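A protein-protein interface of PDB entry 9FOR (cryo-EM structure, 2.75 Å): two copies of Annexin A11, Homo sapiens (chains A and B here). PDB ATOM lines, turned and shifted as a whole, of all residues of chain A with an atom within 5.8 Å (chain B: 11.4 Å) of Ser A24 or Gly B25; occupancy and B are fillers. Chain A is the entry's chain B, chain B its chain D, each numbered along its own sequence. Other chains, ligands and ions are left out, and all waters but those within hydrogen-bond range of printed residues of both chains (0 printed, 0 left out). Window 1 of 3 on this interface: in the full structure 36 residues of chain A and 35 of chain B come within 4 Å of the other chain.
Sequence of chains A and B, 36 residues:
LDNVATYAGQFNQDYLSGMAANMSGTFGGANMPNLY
The side-chain hydroxyl (OG1) of Thr B26 sits at hydrogen-bond distance from the side-chain hydroxyl (OG1) of Thr B6 (2.8 Å).
OG1 of Thr A6 lies within hydrogen-bond range of OG1 of Thr A26 (2.8 Å).
The backbone NH of Ala A8 is in hydrogen-bond range of the backbone carbonyl oxygen of Tyr B7 (3.1 Å).
O of Ser A24 sits at hydrogen-bond distance from N of Gly B25 (3.2 Å).
O of Thr A6 lies within hydrogen-bond range of N of Tyr B7 (3.0 Å).
The backbone NH (N) of Phe A11 is in hydrogen-bond range of the backbone carbonyl oxygen (O) of Gln B10.
The backbone NH of Gly B9 lies within hydrogen-bond range of the backbone carbonyl oxygen of Ala A8 (3.3 Å).
The backbone NH of Thr A26 lies within hydrogen-bond range of the backbone carbonyl oxygen of Gly B25.
O of Ala B5 sits at hydrogen-bond distance from N of Thr A6, at 3.4 Å.
The backbone NH (N) of Asn A22 sits at hydrogen-bond distance from the backbone carbonyl oxygen (O) of Ala B21.
O of Thr A26 is in hydrogen-bond range of N of Phe B27 (3.1 Å).
The side-chain hydroxyl (OG1) of Thr B6 is in hydrogen-bond range of the side-chain hydroxyl (OG1) of Thr A26, at 2.8 Å.
N of Met B23 is in hydrogen-bond range of O of Asn A22 (3.2 Å).
The backbone NH (N) of Ser A24 sits at hydrogen-bond distance from the backbone carbonyl oxygen (O) of Met B23.
OG1 of Thr A26 sits at hydrogen-bond distance from O of Ala B5 (3.3 Å).
Asn A22 touches Met B23, but with the chains exchanged Met A23 does not touch Asn B22 (5.9 Å).
Met B23 touches its own counterpart, Met A23.
Thr A26 touches Thr B6, but with the chains exchanged Thr A6 does not touch Thr B26 (7.7 Å).
Thr A26 touches its own counterpart, Thr B26.
Of the 22 pairs that touch across the chains among the printed residues, 8 have their exchanged pair printed and touching as well.
CA of Thr B6 touches O of Thr A6, at 3.8 Å.
Ala A8 touches Ala B8 (O to CA, 3.5 Å).
Phe B11 touches Phe A11 (CE2 to CD1, 3.6 Å).
Asn B22 touches Asn A22 (OD1 to ND2, 3.5 Å).
CA of Met A23 touches O of Met B23 (3.6 Å).
O of Ser A24 touches CA of Ser B24 (3.5 Å).
CA of Gly A25 touches O of Gly B25, at 3.4 Å.
Thr A26 touches Val B4.
Thr A26 touches Thr B26 (O to CA, 3.7 Å).
Of chain B, only Met B23 (3.1 Å), Ser B24 (3.5 Å) and Gly B25 (3.2 Å) come within 4 Å of Ser A24.
Gly B25 touches just these residues of chain A: Ser A24, Gly A25 and Thr A26.
Met A23 touches one residue of chain B.
Thr A26 touches six residues of chain B.
Printed residues of chain A within 4 Å of Thr B6: Thr A6 and Thr A26.
Printed residues of chain A within 4 Å of Gly B9: Ala A8.
Of the printed residues of chain A, Ser B24 touches Ser A24 (3.5 Å).
Printed residues of chain B within 4 Å of Thr A6: Ala B5 (3.4 Å), Thr B6 (3.8 Å) and Tyr B7 (3.0 Å).
Printed residues of chain A within 4 Å of Ala B8: Ala A8.
The nearest residue of chain B that does not touch Ser A24 is Thr B6 (4.2 Å).
The nearest printed residue of chain A that does not touch Gly B25 is Met A23 (6.8 Å).
Hydrophobic or aromatic side chains of chain A within 4 Å of the printed part of chain B: Phe A11.
Along chain A the printed residues that touch a printed residue of chain B span positions 6 to 26.
Of the 17 printed residues of chain B, 15 touch a printed residue of chain A.
Hydrophobic or aromatic side chains of chain B that line the printed part of chain A: Val B4, Tyr B7, Phe B11 and Phe B27.
Among the printed residues, 22 pairs touch across the chains.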
ATOM      1  N   THR A   6       2.644 -11.882  16.130  1.00  0.00           N
ATOM      2  CA  THR A   6       3.300 -12.931  16.914  1.00  0.00           C
ATOM      3  C   THR A   6       2.465 -13.232  18.155  1.00  0.00           C
ATOM      4  O   THR A   6       2.129 -12.308  18.880  1.00  0.00           O
ATOM      5  CB  THR A   6       4.693 -12.453  17.347  1.00  0.00           C
ATOM      6  OG1 THR A   6       5.474 -12.060  16.223  1.00  0.00           O
ATOM      7  CG2 THR A   6       5.492 -13.512  18.082  1.00  0.00           C
ATOM      8  N   ALA A   8       2.633 -15.590  21.688  1.00  0.00           N
ATOM      9  CA  ALA A   8       3.421 -16.502  22.522  1.00  0.00           C
ATOM     10  C   ALA A   8       2.790 -16.620  23.903  1.00  0.00           C
ATOM     11  O   ALA A   8       2.422 -15.596  24.461  1.00  0.00           O
ATOM     12  CB  ALA A   8       4.816 -15.968  22.665  1.00  0.00           C
ATOM     13  N   PHE A  11       4.030 -18.972  30.072  1.00  0.00           N
ATOM     14  CA  PHE A  11       5.295 -19.482  30.550  1.00  0.00           C
ATOM     15  C   PHE A  11       5.108 -19.988  31.989  1.00  0.00           C
ATOM     16  O   PHE A  11       4.750 -19.209  32.861  1.00  0.00           O
ATOM     17  CB  PHE A  11       6.242 -18.300  30.343  1.00  0.00           C
ATOM     18  CG  PHE A  11       6.363 -17.752  28.927  1.00  0.00           C
ATOM     19  CD1 PHE A  11       5.518 -16.742  28.462  1.00  0.00           C
ATOM     20  CD2 PHE A  11       7.381 -18.196  28.070  1.00  0.00           C
ATOM     21  CE1 PHE A  11       5.675 -16.196  27.166  1.00  0.00           C
ATOM     22  CE2 PHE A  11       7.506 -17.687  26.769  1.00  0.00           C
ATOM     23  CZ  PHE A  11       6.649 -16.683  26.311  1.00  0.00           C
ATOM     24  N   ASN A  22      12.887 -15.283  27.648  1.00  0.00           N
ATOM     25  CA  ASN A  22      11.598 -15.376  26.959  1.00  0.00           C
ATOM     26  C   ASN A  22      11.452 -14.211  25.985  1.00  0.00           C
ATOM     27  O   ASN A  22      10.955 -13.176  26.392  1.00  0.00           O
ATOM     28  CB  ASN A  22      10.477 -15.477  27.997  1.00  0.00           C
ATOM     29  CG  ASN A  22      10.759 -16.604  28.980  1.00  0.00           C
ATOM     30  OD1 ASN A  22      11.545 -17.498  28.660  1.00  0.00           O
ATOM     31  ND2 ASN A  22      10.193 -16.613  30.178  1.00  0.00           N
ATOM     32  N   MET A  23      11.870 -14.338  24.716  1.00  0.00           N
ATOM     33  CA  MET A  23      11.975 -13.173  23.825  1.00  0.00           C
ATOM     34  C   MET A  23      11.017 -13.226  22.625  1.00  0.00           C
ATOM     35  O   MET A  23      11.121 -14.116  21.797  1.00  0.00           O
ATOM     36  CB  MET A  23      13.390 -13.073  23.235  1.00  0.00           C
ATOM     37  CG  MET A  23      14.511 -12.953  24.275  1.00  0.00           C
ATOM     38  SD  MET A  23      16.186 -12.930  23.573  1.00  0.00           S
ATOM     39  CE  MET A  23      16.219 -11.353  22.710  1.00  0.00           C
ATOM     40  N   SER A  24      10.167 -12.210  22.441  1.00  0.00           N
ATOM     41  CA  SER A  24       9.198 -12.157  21.344  1.00  0.00           C
ATOM     42  C   SER A  24       9.356 -10.864  20.557  1.00  0.00           C
ATOM     43  O   SER A  24       9.303  -9.817  21.170  1.00  0.00           O
ATOM     44  CB  SER A  24       7.793 -12.228  21.881  1.00  0.00           C
ATOM     45  OG  SER A  24       7.715 -13.121  22.992  1.00  0.00           O
ATOM     46  N   GLY A  25       9.504 -10.939  19.230  1.00  0.00           N
ATOM     47  CA  GLY A  25       9.735  -9.780  18.382  1.00  0.00           C
ATOM     48  C   GLY A  25       8.967  -9.833  17.050  1.00  0.00           C
ATOM     49  O   GLY A  25       8.805 -10.901  16.466  1.00  0.00           O
ATOM     50  N   THR A  26       8.531  -8.656  16.566  1.00  0.00           N
ATOM     51  CA  THR A  26       7.733  -8.502  15.361  1.00  0.00           C
ATOM     52  C   THR A  26       8.283  -7.333  14.555  1.00  0.00           C
ATOM     53  O   THR A  26       8.464  -6.262  15.108  1.00  0.00           O
ATOM     54  CB  THR A  26       6.266  -8.232  15.722  1.00  0.00           C
ATOM     55  OG1 THR A  26       5.827  -9.271  16.588  1.00  0.00           O
ATOM     56  CG2 THR A  26       5.353  -8.243  14.506  1.00  0.00           C
ATOM     57  N   VAL B   4       0.555  -4.176  12.756  1.00  0.00           N
ATOM     58  CA  VAL B   4       1.753  -4.858  13.235  1.00  0.00           C
ATOM     59  C   VAL B   4       1.684  -4.986  14.750  1.00  0.00           C
ATOM     60  O   VAL B   4       1.748  -3.964  15.421  1.00  0.00           O
ATOM     61  CB  VAL B   4       3.014  -4.055  12.866  1.00  0.00           C
ATOM     62  CG1 VAL B   4       4.289  -4.728  13.326  1.00  0.00           C
ATOM     63  CG2 VAL B   4       3.123  -3.785  11.392  1.00  0.00           C
ATOM     64  N   ALA B   5       1.666  -6.207  15.296  1.00  0.00           N
ATOM     65  CA  ALA B   5       1.406  -6.381  16.720  1.00  0.00           C
ATOM     66  C   ALA B   5       2.138  -7.572  17.356  1.00  0.00           C
ATOM     67  O   ALA B   5       2.577  -8.480  16.659  1.00  0.00           O
ATOM     68  CB  ALA B   5      -0.070  -6.513  16.886  1.00  0.00           C
ATOM     69  N   THR B   6       2.241  -7.566  18.703  1.00  0.00           N
ATOM     70  CA  THR B   6       2.857  -8.630  19.499  1.00  0.00           C
ATOM     71  C   THR B   6       1.987  -8.916  20.720  1.00  0.00           C
ATOM     72  O   THR B   6       1.651  -7.986  21.439  1.00  0.00           O
ATOM     73  CB  THR B   6       4.249  -8.180  19.968  1.00  0.00           C
ATOM     74  OG1 THR B   6       5.064  -7.802  18.865  1.00  0.00           O
ATOM     75  CG2 THR B   6       5.007  -9.257  20.720  1.00  0.00           C
ATOM     76  N   TYR B   7       1.692 -10.184  21.014  1.00  0.00           N
ATOM     77  CA  TYR B   7       0.886 -10.532  22.183  1.00  0.00           C
ATOM     78  C   TYR B   7       1.590 -11.609  23.028  1.00  0.00           C
ATOM     79  O   TYR B   7       1.726 -12.747  22.595  1.00  0.00           O
ATOM     80  CB  TYR B   7      -0.485 -11.040  21.722  1.00  0.00           C
ATOM     81  CG  TYR B   7      -1.232 -10.251  20.656  1.00  0.00           C
ATOM     82  CD1 TYR B   7      -0.917 -10.364  19.309  1.00  0.00           C
ATOM     83  CD2 TYR B   7      -2.323  -9.450  20.984  1.00  0.00           C
ATOM     84  CE1 TYR B   7      -1.605  -9.651  18.334  1.00  0.00           C
ATOM     85  CE2 TYR B   7      -3.035  -8.748  20.022  1.00  0.00           C
ATOM     86  CZ  TYR B   7      -2.674  -8.843  18.688  1.00  0.00           C
ATOM     87  OH  TYR B   7      -3.351  -8.138  17.730  1.00  0.00           O
ATOM     88  N   ALA B   8       2.019 -11.282  24.251  1.00  0.00           N
ATOM     89  CA  ALA B   8       2.767 -12.211  25.101  1.00  0.00           C
ATOM     90  C   ALA B   8       2.101 -12.320  26.466  1.00  0.00           C
ATOM     91  O   ALA B   8       1.741 -11.289  27.017  1.00  0.00           O
ATOM     92  CB  ALA B   8       4.170 -11.707  25.280  1.00  0.00           C
ATOM     93  N   GLY B   9       1.934 -13.524  27.026  1.00  0.00           N
ATOM     94  CA  GLY B   9       0.815 -13.685  27.949  1.00  0.00           C
ATOM     95  C   GLY B   9       1.036 -14.654  29.102  1.00  0.00           C
ATOM     96  O   GLY B   9       1.326 -15.815  28.886  1.00  0.00           O
ATOM     97  N   GLN B  10       0.766 -14.162  30.311  1.00  0.00           N
ATOM     98  CA  GLN B  10       0.993 -14.854  31.563  1.00  0.00           C
ATOM     99  C   GLN B  10       2.438 -15.316  31.704  1.00  0.00           C
ATOM    100  O   GLN B  10       2.862 -16.238  31.025  1.00  0.00           O
ATOM    101  CB  GLN B  10       0.006 -15.989  31.755  1.00  0.00           C
ATOM    102  CG  GLN B  10      -1.136 -15.604  32.677  1.00  0.00           C
ATOM    103  CD  GLN B  10      -1.506 -16.709  33.632  1.00  0.00           C
ATOM    104  OE1 GLN B  10      -0.979 -17.823  33.568  1.00  0.00           O
ATOM    105  NE2 GLN B  10      -2.446 -16.419  34.514  1.00  0.00           N
ATOM    106  N   PHE B  11       3.140 -14.707  32.659  1.00  0.00           N
ATOM    107  CA  PHE B  11       4.383 -15.243  33.167  1.00  0.00           C
ATOM    108  C   PHE B  11       4.151 -15.747  34.599  1.00  0.00           C
ATOM    109  O   PHE B  11       3.787 -14.963  35.464  1.00  0.00           O
ATOM    110  CB  PHE B  11       5.360 -14.080  32.986  1.00  0.00           C
ATOM    111  CG  PHE B  11       5.526 -13.533  31.574  1.00  0.00           C
ATOM    112  CD1 PHE B  11       4.713 -12.504  31.091  1.00  0.00           C
ATOM    113  CD2 PHE B  11       6.556 -13.995  30.741  1.00  0.00           C
ATOM    114  CE1 PHE B  11       4.914 -11.960  29.801  1.00  0.00           C
ATOM    115  CE2 PHE B  11       6.723 -13.488  29.445  1.00  0.00           C
ATOM    116  CZ  PHE B  11       5.898 -12.465  28.968  1.00  0.00           C
ATOM    117  N   ALA B  21      14.707 -12.949  31.869  1.00  0.00           N
ATOM    118  CA  ALA B  21      14.459 -11.806  31.006  1.00  0.00           C
ATOM    119  C   ALA B  21      13.166 -12.011  30.200  1.00  0.00           C
ATOM    120  O   ALA B  21      13.107 -12.892  29.348  1.00  0.00           O
ATOM    121  CB  ALA B  21      15.656 -11.638  30.099  1.00  0.00           C
ATOM    122  N   ASN B  22      12.128 -11.195  30.460  1.00  0.00           N
ATOM    123  CA  ASN B  22      10.854 -11.260  29.741  1.00  0.00           C
ATOM    124  C   ASN B  22      10.756 -10.091  28.766  1.00  0.00           C
ATOM    125  O   ASN B  22      10.270  -9.047  29.162  1.00  0.00           O
ATOM    126  CB  ASN B  22       9.707 -11.340  30.750  1.00  0.00           C
ATOM    127  CG  ASN B  22       9.942 -12.475  31.737  1.00  0.00           C
ATOM    128  OD1 ASN B  22      10.717 -13.383  31.435  1.00  0.00           O
ATOM    129  ND2 ASN B  22       9.346 -12.474  32.921  1.00  0.00           N
ATOM    130  N   MET B  23      11.203 -10.223  27.506  1.00  0.00           N
ATOM    131  CA  MET B  23      11.353  -9.060  26.621  1.00  0.00           C
ATOM    132  C   MET B  23      10.423  -9.092  25.398  1.00  0.00           C
ATOM    133  O   MET B  23      10.530  -9.982  24.570  1.00  0.00           O
ATOM    134  CB  MET B  23      12.784  -8.988  26.067  1.00  0.00           C
ATOM    135  CG  MET B  23      13.882  -8.892  27.134  1.00  0.00           C
ATOM    136  SD  MET B  23      15.573  -8.903  26.473  1.00  0.00           S
ATOM    137  CE  MET B  23      15.660  -7.325  25.615  1.00  0.00           C
ATOM    138  N   SER B  24       9.600  -8.057  25.195  1.00  0.00           N
ATOM    139  CA  SER B  24       8.659  -7.983  24.075  1.00  0.00           C
ATOM    140  C   SER B  24       8.864  -6.693  23.295  1.00  0.00           C
ATOM    141  O   SER B  24       8.816  -5.645  23.909  1.00  0.00           O
ATOM    142  CB  SER B  24       7.241  -8.026  24.578  1.00  0.00           C
ATOM    143  OG  SER B  24       7.116  -8.920  25.684  1.00  0.00           O
ATOM    144  N   GLY B  25       9.041  -6.769  21.972  1.00  0.00           N
ATOM    145  CA  GLY B  25       9.317  -5.613  21.133  1.00  0.00           C
ATOM    146  C   GLY B  25       8.581  -5.648  19.782  1.00  0.00           C
ATOM    147  O   GLY B  25       8.411  -6.711  19.192  1.00  0.00           O
ATOM    148  N   THR B  26       8.181  -4.461  19.289  1.00  0.00           N
ATOM    149  CA  THR B  26       7.416  -4.290  18.067  1.00  0.00           C
ATOM    150  C   THR B  26       8.009  -3.131  17.277  1.00  0.00           C
ATOM    151  O   THR B  26       8.198  -2.064  17.836  1.00  0.00           O
ATOM    152  CB  THR B  26       5.946  -3.990  18.392  1.00  0.00           C
ATOM    153  OG1 THR B  26       5.466  -5.021  19.244  1.00  0.00           O
ATOM    154  CG2 THR B  26       5.064  -3.980  17.153  1.00  0.00           C
ATOM    155  N   PHE B  27       8.202  -3.289  15.962  1.00  0.00           N
ATOM    156  CA  PHE B  27       8.919  -2.286  15.181  1.00  0.00           C
ATOM    157  C   PHE B  27       8.207  -2.036  13.866  1.00  0.00           C
ATOM    158  O   PHE B  27       8.199  -2.899  13.012  1.00  0.00           O
ATOM    159  CB  PHE B  27      10.353  -2.728  14.871  1.00  0.00           C
ATOM    160  CG  PHE B  27      11.185  -3.036  16.104  1.00  0.00           C
ATOM    161  CD1 PHE B  27      11.077  -4.268  16.740  1.00  0.00           C
ATOM    162  CD2 PHE B  27      12.059  -2.094  16.641  1.00  0.00           C
ATOM    163  CE1 PHE B  27      11.807  -4.546  17.898  1.00  0.00           C
ATOM    164  CE2 PHE B  27      12.815  -2.385  17.776  1.00  0.00           C
ATOM    165  CZ  PHE B  27      12.683  -3.606  18.409  1.00  0.00           C
ATOM    166  N   GLY B  28       7.645  -0.855  13.681  1.00  0.00           N
ATOM    167  CA  GLY B  28       6.905  -0.568  12.466  1.00  0.00           C
ATOM    168  C   GLY B  28       7.850  -0.591  11.289  1.00  0.00           C
ATOM    169  O   GLY B  28       9.057  -0.510  11.488  1.00  0.00           O
ATOM    170  N   GLY B  29       7.316  -0.668  10.069  1.00  0.00           N
ATOM    171  CA  GLY B  29       8.229  -0.703   8.949  1.00  0.00           C
ATOM    172  C   GLY B  29       7.643  -0.231   7.634  1.00  0.00           C
ATOM    173  O   GLY B  29       6.972  -0.993   6.947  1.00  0.00           O
